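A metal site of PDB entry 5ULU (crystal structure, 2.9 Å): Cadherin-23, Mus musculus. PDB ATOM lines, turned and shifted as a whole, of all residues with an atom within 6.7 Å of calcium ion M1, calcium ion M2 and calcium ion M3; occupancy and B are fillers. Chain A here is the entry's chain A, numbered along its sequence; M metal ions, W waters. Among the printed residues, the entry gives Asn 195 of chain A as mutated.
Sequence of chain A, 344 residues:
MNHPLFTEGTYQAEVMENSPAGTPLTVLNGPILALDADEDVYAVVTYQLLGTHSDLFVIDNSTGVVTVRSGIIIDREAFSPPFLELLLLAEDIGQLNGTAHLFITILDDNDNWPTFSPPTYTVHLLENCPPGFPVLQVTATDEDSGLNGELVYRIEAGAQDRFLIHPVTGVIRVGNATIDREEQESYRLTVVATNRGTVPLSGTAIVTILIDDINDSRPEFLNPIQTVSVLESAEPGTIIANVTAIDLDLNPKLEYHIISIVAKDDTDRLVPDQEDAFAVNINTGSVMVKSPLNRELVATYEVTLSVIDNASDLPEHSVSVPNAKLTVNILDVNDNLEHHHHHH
Six residues have an atom within 4 Å of calcium ion M3: Asn 110, Asn 112, Asp 142, Asp 144, Asn 148 and Asn 195. The nearest printed residue that does not touch calcium ion M3 is Pro 114 (4.3 Å).
The backbone carbonyl oxygen (O) of Val 199 sits at hydrogen-bond distance from the side-chain amide nitrogen (ND2) of Asn 110, at 2.7 Å. OD2 of Asp 111 lies close to ND2 of Asn 18. ND2 of Asn 18 lies within hydrogen-bond range of OD2 of Asp 109 (3.2 Å). OE1 of Glu 77 sits close to NH2 of Arg 76. N of Arg 76 sits close to OE2 of Glu 17 (3.2 Å). NE of Arg 76 lies close to OD1 of Asp 108, 3.2 Å away. The side-chain carboxylate (OD1) of Asp 111 sits close to the side-chain amide nitrogen (ND2) of Asn 112 (3.0 Å). N of Ser 145 sits at hydrogen-bond distance from OD2 of Asp 108 (3.1 Å).
Calcium ion M3 is bound by the side-chain amide oxygen (OD1) of Asn 110 (2.1 Å), the backbone carbonyl oxygen (O) of Asn 112 (2.2 Å), the side-chain carboxylate (OD2) of Asp 144 (2.2 Å), the side-chain carboxylate (OD1) of Asp 142 (2.4 Å), the side-chain carboxylate (OD2) of Asp 142 (2.4 Å), the backbone carbonyl oxygen (O) of Asn 148 (2.5 Å) and the side-chain amide oxygen (OD1) of Asn 195 (2.5 Å).
Along chain A the residues within 4 Å of calcium ion M1 span positions 17 to 144.
Water W2 binds calcium ion M2, 2.1 Å away. Calcium ion M2 is bound by OE2 of Glu 77, at 2.3 Å. Calcium ion M2 is bound by water W1, 2.4 Å away. The side-chain carboxylate (OE2) of Glu 17 binds calcium ion M2 (2.5 Å). The side-chain carboxylate (OD1) of Asp 75 binds calcium ion M2. OD2 of Asp 111 is bound to calcium ion M2 (2.7 Å). Calcium ion M2 has six donor atoms within binding distance. Slightly farther from calcium ion M2 lies the side-chain carboxylate (OD1) of Asp 111 (2.9 Å).
OE1 of Glu 17 binds calcium ion M1. The backbone carbonyl oxygen (O) of Asp 109 binds calcium ion M1 (2.3 Å). Calcium ion M1 is bound by the side-chain carboxylate (OD1) of Asp 108, at 2.3 Å. The side-chain carboxylate (OD1) of Asp 144 is bound to calcium ion M1, 2.3 Å away. Calcium ion M1 is bound by OE2 of Glu 77, 2.4 Å away. OD1 of Asp 111 is bound to calcium ion M1 (2.6 Å). Calcium ion M1 is bound by OE1 of Glu 77 (2.6 Å).
Water W1 lies within hydrogen-bond range of ND2 of Asn 112 and O of Asp 111.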
ATOM      1  N   GLU A  17     -13.657   2.196  24.917  1.00  0.00           N
ATOM      2  CA  GLU A  17     -14.876   1.378  24.960  1.00  0.00           C
ATOM      3  C   GLU A  17     -14.821   0.288  23.895  1.00  0.00           C
ATOM      4  O   GLU A  17     -14.145   0.438  22.862  1.00  0.00           O
ATOM      5  CB  GLU A  17     -16.164   2.227  24.815  1.00  0.00           C
ATOM      6  CG  GLU A  17     -16.257   3.163  23.621  1.00  0.00           C
ATOM      7  CD  GLU A  17     -17.693   3.557  23.250  1.00  0.00           C
ATOM      8  OE1 GLU A  17     -17.844   4.644  22.631  1.00  0.00           O
ATOM      9  OE2 GLU A  17     -18.655   2.788  23.535  1.00  0.00           O
ATOM     10  N   ASN A  18     -15.482  -0.835  24.173  1.00  0.00           N
ATOM     11  CA  ASN A  18     -15.546  -1.990  23.247  1.00  0.00           C
ATOM     12  C   ASN A  18     -14.265  -2.810  23.174  1.00  0.00           C
ATOM     13  O   ASN A  18     -14.275  -3.842  22.512  1.00  0.00           O
ATOM     14  CB  ASN A  18     -15.964  -1.584  21.812  1.00  0.00           C
ATOM     15  CG  ASN A  18     -17.291  -0.857  21.758  1.00  0.00           C
ATOM     16  OD1 ASN A  18     -18.286  -1.348  22.265  1.00  0.00           O
ATOM     17  ND2 ASN A  18     -17.313   0.332  21.125  1.00  0.00           N
ATOM     18  N   ILE A  74     -17.830  -3.067  27.372  1.00  0.00           N
ATOM     19  CA  ILE A  74     -17.640  -1.725  27.951  1.00  0.00           C
ATOM     20  C   ILE A  74     -18.149  -0.619  27.007  1.00  0.00           C
ATOM     21  O   ILE A  74     -17.444  -0.195  26.089  1.00  0.00           O
ATOM     22  CB  ILE A  74     -16.150  -1.487  28.299  1.00  0.00           C
ATOM     23  CG1 ILE A  74     -15.659  -2.556  29.273  1.00  0.00           C
ATOM     24  CG2 ILE A  74     -15.945  -0.096  28.903  1.00  0.00           C
ATOM     25  CD1 ILE A  74     -14.220  -2.362  29.716  1.00  0.00           C
ATOM     26  N   ASP A  75     -19.360  -0.135  27.285  1.00  0.00           N
ATOM     27  CA  ASP A  75     -20.021   0.917  26.506  1.00  0.00           C
ATOM     28  C   ASP A  75     -19.872   2.288  27.202  1.00  0.00           C
ATOM     29  O   ASP A  75     -20.505   2.523  28.223  1.00  0.00           O
ATOM     30  CB  ASP A  75     -21.507   0.552  26.339  1.00  0.00           C
ATOM     31  CG  ASP A  75     -22.261   1.526  25.446  1.00  0.00           C
ATOM     32  OD1 ASP A  75     -21.734   2.579  25.102  1.00  0.00           O
ATOM     33  OD2 ASP A  75     -23.395   1.212  25.067  1.00  0.00           O
ATOM     34  N   ARG A  76     -19.075   3.200  26.632  1.00  0.00           N
ATOM     35  CA  ARG A  76     -18.990   4.566  27.121  1.00  0.00           C
ATOM     36  C   ARG A  76     -20.362   5.221  27.210  1.00  0.00           C
ATOM     37  O   ARG A  76     -20.648   5.940  28.153  1.00  0.00           O
ATOM     38  CB  ARG A  76     -18.122   5.440  26.239  1.00  0.00           C
ATOM     39  CG  ARG A  76     -17.629   6.686  26.984  1.00  0.00           C
ATOM     40  CD  ARG A  76     -17.191   7.847  26.102  1.00  0.00           C
ATOM     41  NE  ARG A  76     -18.265   8.288  25.224  1.00  0.00           N
ATOM     42  CZ  ARG A  76     -19.295   9.058  25.584  1.00  0.00           C
ATOM     43  NH1 ARG A  76     -19.423   9.483  26.843  1.00  0.00           N
ATOM     44  NH2 ARG A  76     -20.215   9.386  24.685  1.00  0.00           N
ATOM     45  N   GLU A  77     -21.216   4.948  26.234  1.00  0.00           N
ATOM     46  CA  GLU A  77     -22.556   5.525  26.188  1.00  0.00           C
ATOM     47  C   GLU A  77     -23.470   5.086  27.362  1.00  0.00           C
ATOM     48  O   GLU A  77     -24.532   5.629  27.544  1.00  0.00           O
ATOM     49  CB  GLU A  77     -23.213   5.216  24.831  1.00  0.00           C
ATOM     50  CG  GLU A  77     -22.748   6.104  23.675  1.00  0.00           C
ATOM     51  CD  GLU A  77     -21.263   6.017  23.351  1.00  0.00           C
ATOM     52  OE1 GLU A  77     -20.603   7.075  23.369  1.00  0.00           O
ATOM     53  OE2 GLU A  77     -20.739   4.903  23.042  1.00  0.00           O
ATOM     54  N   ALA A  78     -23.040   4.084  28.129  1.00  0.00           N
ATOM     55  CA  ALA A  78     -23.775   3.600  29.300  1.00  0.00           C
ATOM     56  C   ALA A  78     -23.230   4.096  30.650  1.00  0.00           C
ATOM     57  O   ALA A  78     -23.731   3.688  31.676  1.00  0.00           O
ATOM     58  CB  ALA A  78     -23.792   2.076  29.284  1.00  0.00           C
ATOM     59  N   LEU A 107     -12.582   6.008  27.099  1.00  0.00           N
ATOM     60  CA  LEU A 107     -12.514   6.776  25.861  1.00  0.00           C
ATOM     61  C   LEU A 107     -13.621   6.410  24.844  1.00  0.00           C
ATOM     62  O   LEU A 107     -14.139   5.253  24.838  1.00  0.00           O
ATOM     63  CB  LEU A 107     -11.138   6.636  25.228  1.00  0.00           C
ATOM     64  CG  LEU A 107      -9.985   7.224  26.046  1.00  0.00           C
ATOM     65  CD1 LEU A 107      -8.670   6.745  25.460  1.00  0.00           C
ATOM     66  CD2 LEU A 107     -10.032   8.759  26.140  1.00  0.00           C
ATOM     67  N   ASP A 108     -13.956   7.392  23.992  1.00  0.00           N
ATOM     68  CA  ASP A 108     -15.106   7.299  23.098  1.00  0.00           C
ATOM     69  C   ASP A 108     -14.728   6.676  21.745  1.00  0.00           C
ATOM     70  O   ASP A 108     -13.710   7.003  21.121  1.00  0.00           O
ATOM     71  CB  ASP A 108     -15.726   8.689  22.904  1.00  0.00           C
ATOM     72  CG  ASP A 108     -16.989   8.662  22.049  1.00  0.00           C
ATOM     73  OD1 ASP A 108     -17.778   7.695  22.143  1.00  0.00           O
ATOM     74  OD2 ASP A 108     -17.198   9.653  21.302  1.00  0.00           O
ATOM     75  N   ASP A 109     -15.579   5.766  21.318  1.00  0.00           N
ATOM     76  CA  ASP A 109     -15.524   5.174  20.007  1.00  0.00           C
ATOM     77  C   ASP A 109     -16.638   5.795  19.209  1.00  0.00           C
ATOM     78  O   ASP A 109     -17.678   6.140  19.765  1.00  0.00           O
ATOM     79  CB  ASP A 109     -15.772   3.676  20.143  1.00  0.00           C
ATOM     80  CG  ASP A 109     -15.087   2.863  19.099  1.00  0.00           C
ATOM     81  OD1 ASP A 109     -14.112   3.385  18.530  1.00  0.00           O
ATOM     82  OD2 ASP A 109     -15.509   1.699  18.885  1.00  0.00           O
ATOM     83  N   ASN A 110     -16.453   5.962  17.896  1.00  0.00           N
ATOM     84  CA  ASN A 110     -17.570   6.395  17.051  1.00  0.00           C
ATOM     85  C   ASN A 110     -18.393   5.170  16.651  1.00  0.00           C
ATOM     86  O   ASN A 110     -18.283   4.650  15.528  1.00  0.00           O
ATOM     87  CB  ASN A 110     -17.103   7.197  15.839  1.00  0.00           C
ATOM     88  CG  ASN A 110     -18.226   8.004  15.208  1.00  0.00           C
ATOM     89  OD1 ASN A 110     -19.329   8.080  15.770  1.00  0.00           O
ATOM     90  ND2 ASN A 110     -17.960   8.611  14.055  1.00  0.00           N
ATOM     91  N   ASP A 111     -19.239   4.721  17.586  1.00  0.00           N
ATOM     92  CA  ASP A 111     -20.070   3.534  17.362  1.00  0.00           C
ATOM     93  C   ASP A 111     -21.577   3.843  17.332  1.00  0.00           C
ATOM     94  O   ASP A 111     -22.429   2.964  17.570  1.00  0.00           O
ATOM     95  CB  ASP A 111     -19.721   2.419  18.350  1.00  0.00           C
ATOM     96  CG  ASP A 111     -19.714   2.863  19.783  1.00  0.00           C
ATOM     97  OD1 ASP A 111     -20.135   3.999  20.102  1.00  0.00           O
ATOM     98  OD2 ASP A 111     -19.287   2.044  20.601  1.00  0.00           O
ATOM     99  N   ASN A 112     -21.898   5.081  16.967  1.00  0.00           N
ATOM    100  CA  ASN A 112     -23.264   5.481  16.843  1.00  0.00           C
ATOM    101  C   ASN A 112     -23.427   6.383  15.614  1.00  0.00           C
ATOM    102  O   ASN A 112     -22.721   7.393  15.470  1.00  0.00           O
ATOM    103  CB  ASN A 112     -23.749   6.190  18.141  1.00  0.00           C
ATOM    104  CG  ASN A 112     -23.842   5.241  19.331  1.00  0.00           C
ATOM    105  OD1 ASN A 112     -24.773   4.462  19.422  1.00  0.00           O
ATOM    106  ND2 ASN A 112     -22.832   5.253  20.196  1.00  0.00           N
ATOM    107  N   TRP A 113     -24.378   6.015  14.757  1.00  0.00           N
ATOM    108  CA  TRP A 113     -24.569   6.685  13.485  1.00  0.00           C
ATOM    109  C   TRP A 113     -25.421   7.925  13.711  1.00  0.00           C
ATOM    110  O   TRP A 113     -26.376   7.878  14.473  1.00  0.00           O
ATOM    111  CB  TRP A 113     -25.278   5.779  12.503  1.00  0.00           C
ATOM    112  CG  TRP A 113     -24.392   4.880  11.763  1.00  0.00           C
ATOM    113  CD1 TRP A 113     -24.122   4.915  10.410  1.00  0.00           C
ATOM    114  CD2 TRP A 113     -23.666   3.781  12.283  1.00  0.00           C
ATOM    115  NE1 TRP A 113     -23.240   3.918  10.087  1.00  0.00           N
ATOM    116  CE2 TRP A 113     -22.959   3.203  11.213  1.00  0.00           C
ATOM    117  CE3 TRP A 113     -23.529   3.237  13.558  1.00  0.00           C
ATOM    118  CZ2 TRP A 113     -22.140   2.099  11.372  1.00  0.00           C
ATOM    119  CZ3 TRP A 113     -22.708   2.156  13.722  1.00  0.00           C
ATOM    120  CH2 TRP A 113     -22.032   1.586  12.642  1.00  0.00           C
ATOM    121  N   PRO A 114     -25.088   9.038  13.048  1.00  0.00           N
ATOM    122  CA  PRO A 114     -26.081  10.105  12.911  1.00  0.00           C
ATOM    123  C   PRO A 114     -27.464   9.595  12.507  1.00  0.00           C
ATOM    124  O   PRO A 114     -27.613   8.935  11.464  1.00  0.00           O
ATOM    125  CB  PRO A 114     -25.499  10.985  11.802  1.00  0.00           C
ATOM    126  CG  PRO A 114     -24.126  10.438  11.505  1.00  0.00           C
ATOM    127  CD  PRO A 114     -23.767   9.474  12.583  1.00  0.00           C
ATOM    128  N   ASP A 142     -26.851  11.980  17.623  1.00  0.00           N
ATOM    129  CA  ASP A 142     -25.702  11.088  17.654  1.00  0.00           C
ATOM    130  C   ASP A 142     -25.296  10.902  19.113  1.00  0.00           C
ATOM    131  O   ASP A 142     -24.898  11.843  19.766  1.00  0.00           O
ATOM    132  CB  ASP A 142     -24.548  11.716  16.842  1.00  0.00           C
ATOM    133  CG  ASP A 142     -23.338  10.764  16.615  1.00  0.00           C
ATOM    134  OD1 ASP A 142     -22.752  10.167  17.554  1.00  0.00           O
ATOM    135  OD2 ASP A 142     -22.925  10.641  15.459  1.00  0.00           O
ATOM    136  N   GLU A 143     -25.344   9.669  19.584  1.00  0.00           N
ATOM    137  CA  GLU A 143     -25.093   9.382  20.980  1.00  0.00           C
ATOM    138  C   GLU A 143     -23.620   9.411  21.417  1.00  0.00           C
ATOM    139  O   GLU A 143     -23.317   9.096  22.557  1.00  0.00           O
ATOM    140  CB  GLU A 143     -25.755   8.046  21.361  1.00  0.00           C
ATOM    141  CG  GLU A 143     -27.280   8.020  21.141  1.00  0.00           C
ATOM    142  CD  GLU A 143     -28.071   9.048  21.989  1.00  0.00           C
ATOM    143  OE1 GLU A 143     -27.930   9.047  23.229  1.00  0.00           O
ATOM    144  OE2 GLU A 143     -28.862   9.836  21.402  1.00  0.00           O
ATOM    145  N   ASP A 144     -22.690   9.804  20.556  1.00  0.00           N
ATOM    146  CA  ASP A 144     -21.276   9.870  20.963  1.00  0.00           C
ATOM    147  C   ASP A 144     -20.930  11.265  21.482  1.00  0.00           C
ATOM    148  O   ASP A 144     -21.790  12.155  21.550  1.00  0.00           O
ATOM    149  CB  ASP A 144     -20.375   9.492  19.779  1.00  0.00           C
ATOM    150  CG  ASP A 144     -20.622   8.082  19.250  1.00  0.00           C
ATOM    151  OD1 ASP A 144     -20.431   7.105  20.006  1.00  0.00           O
ATOM    152  OD2 ASP A 144     -20.951   7.956  18.041  1.00  0.00           O
ATOM    153  N   SER A 145     -19.657  11.435  21.848  1.00  0.00           N
ATOM    154  CA  SER A 145     -19.132  12.694  22.419  1.00  0.00           C
ATOM    155  C   SER A 145     -17.955  13.232  21.587  1.00  0.00           C
ATOM    156  O   SER A 145     -17.212  12.449  20.951  1.00  0.00           O
ATOM    157  CB  SER A 145     -18.650  12.439  23.849  1.00  0.00           C
ATOM    158  OG  SER A 145     -17.575  11.501  23.862  1.00  0.00           O
ATOM    159  N   LEU A 147     -15.736  14.925  18.648  1.00  0.00           N
ATOM    160  CA  LEU A 147     -15.679  14.696  17.180  1.00  0.00           C
ATOM    161  C   LEU A 147     -16.652  13.640  16.703  1.00  0.00           C
ATOM    162  O   LEU A 147     -17.362  13.841  15.713  1.00  0.00           O
ATOM    163  CB  LEU A 147     -14.256  14.286  16.751  1.00  0.00           C
ATOM    164  CG  LEU A 147     -13.216  15.422  16.812  1.00  0.00           C
ATOM    165  CD1 LEU A 147     -11.838  14.907  17.221  1.00  0.00           C
ATOM    166  CD2 LEU A 147     -13.185  16.202  15.495  1.00  0.00           C
ATOM    167  N   ASN A 148     -16.679  12.516  17.425  1.00  0.00           N
ATOM    168  CA  ASN A 148     -17.562  11.368  17.130  1.00  0.00           C
ATOM    169  C   ASN A 148     -19.075  11.693  17.191  1.00  0.00           C
ATOM    170  O   ASN A 148     -19.910  11.007  16.570  1.00  0.00           O
ATOM    171  CB  ASN A 148     -17.279  10.227  18.111  1.00  0.00           C
ATOM    172  CG  ASN A 148     -15.879   9.695  18.005  1.00  0.00           C
ATOM    173  OD1 ASN A 148     -15.132  10.065  17.118  1.00  0.00           O
ATOM    174  ND2 ASN A 148     -15.503   8.803  18.926  1.00  0.00           N
ATOM    175  N   GLY A 149     -19.429  12.706  17.962  1.00  0.00           N
ATOM    176  CA  GLY A 149     -20.813  13.078  18.148  1.00  0.00           C
ATOM    177  C   GLY A 149     -21.304  14.241  17.339  1.00  0.00           C
ATOM    178  O   GLY A 149     -22.510  14.485  17.315  1.00  0.00           O
ATOM    179  N   GLU A 150     -20.402  15.001  16.714  1.00  0.00           N
ATOM    180  CA  GLU A 150     -20.807  16.287  16.101  1.00  0.00           C
ATOM    181  C   GLU A 150     -21.181  16.058  14.638  1.00  0.00           C
ATOM    182  O   GLU A 150     -20.885  15.012  14.082  1.00  0.00           O
ATOM    183  CB  GLU A 150     -19.773  17.423  16.325  1.00  0.00           C
ATOM    184  CG  GLU A 150     -18.376  17.225  15.763  1.00  0.00           C
ATOM    185  CD  GLU A 150     -17.426  18.360  16.133  1.00  0.00           C
ATOM    186  OE1 GLU A 150     -17.777  19.526  15.878  1.00  0.00           O
ATOM    187  OE2 GLU A 150     -16.316  18.081  16.666  1.00  0.00           O
ATOM    188  N   ASN A 195     -20.366  12.707  10.941  1.00  0.00           N
ATOM    189  CA  ASN A 195     -19.463  12.911  12.060  1.00  0.00           C
ATOM    190  C   ASN A 195     -18.146  13.373  11.529  1.00  0.00           C
ATOM    191  O   ASN A 195     -17.807  13.110  10.377  1.00  0.00           O
ATOM    192  CB  ASN A 195     -19.240  11.627  12.871  1.00  0.00           C
ATOM    193  CG  ASN A 195     -20.486  11.144  13.595  1.00  0.00           C
ATOM    194  OD1 ASN A 195     -20.671   9.938  13.811  1.00  0.00           O
ATOM    195  ND2 ASN A 195     -21.344  12.091  14.017  1.00  0.00           N
ATOM    196  N   VAL A 199     -13.487   8.354  11.627  1.00  0.00           N
ATOM    197  CA  VAL A 199     -14.559   7.489  11.143  1.00  0.00           C
ATOM    198  C   VAL A 199     -15.810   8.329  10.826  1.00  0.00           C
ATOM    199  O   VAL A 199     -16.674   8.516  11.699  1.00  0.00           O
ATOM    200  CB  VAL A 199     -14.876   6.379  12.178  1.00  0.00           C
ATOM    201  CG1 VAL A 199     -15.991   5.482  11.689  1.00  0.00           C
ATOM    202  CG2 VAL A 199     -13.643   5.556  12.457  1.00  0.00           C
ATOM    203  N   LEU A 201     -19.055   8.611   9.983  1.00  0.00           N
ATOM    204  CA  LEU A 201     -20.354   7.969   9.806  1.00  0.00           C
ATOM    205  C   LEU A 201     -21.341   9.020   9.392  1.00  0.00           C
ATOM    206  O   LEU A 201     -21.273  10.132   9.882  1.00  0.00           O
ATOM    207  CB  LEU A 201     -20.857   7.331  11.088  1.00  0.00           C
ATOM    208  CG  LEU A 201     -19.986   6.300  11.784  1.00  0.00           C
ATOM    209  CD1 LEU A 201     -20.750   5.723  12.980  1.00  0.00           C
ATOM    210  CD2 LEU A 201     -19.559   5.227  10.803  1.00  0.00           C
HETATM  211 CA    CA M   1     -19.132   5.912  21.533  1.00  0.00          CA
HETATM  212 CA    CA M   2     -20.926   2.663  22.602  1.00  0.00          CA
HETATM  213 CA    CA M   3     -21.266   8.953  16.061  1.00  0.00          CA
HETATM  214  O   HOH W   1     -22.692   2.569  20.928  1.00  0.00           O
HETATM  215  O   HOH W   2     -20.203   0.766  23.106  1.00  0.00           O
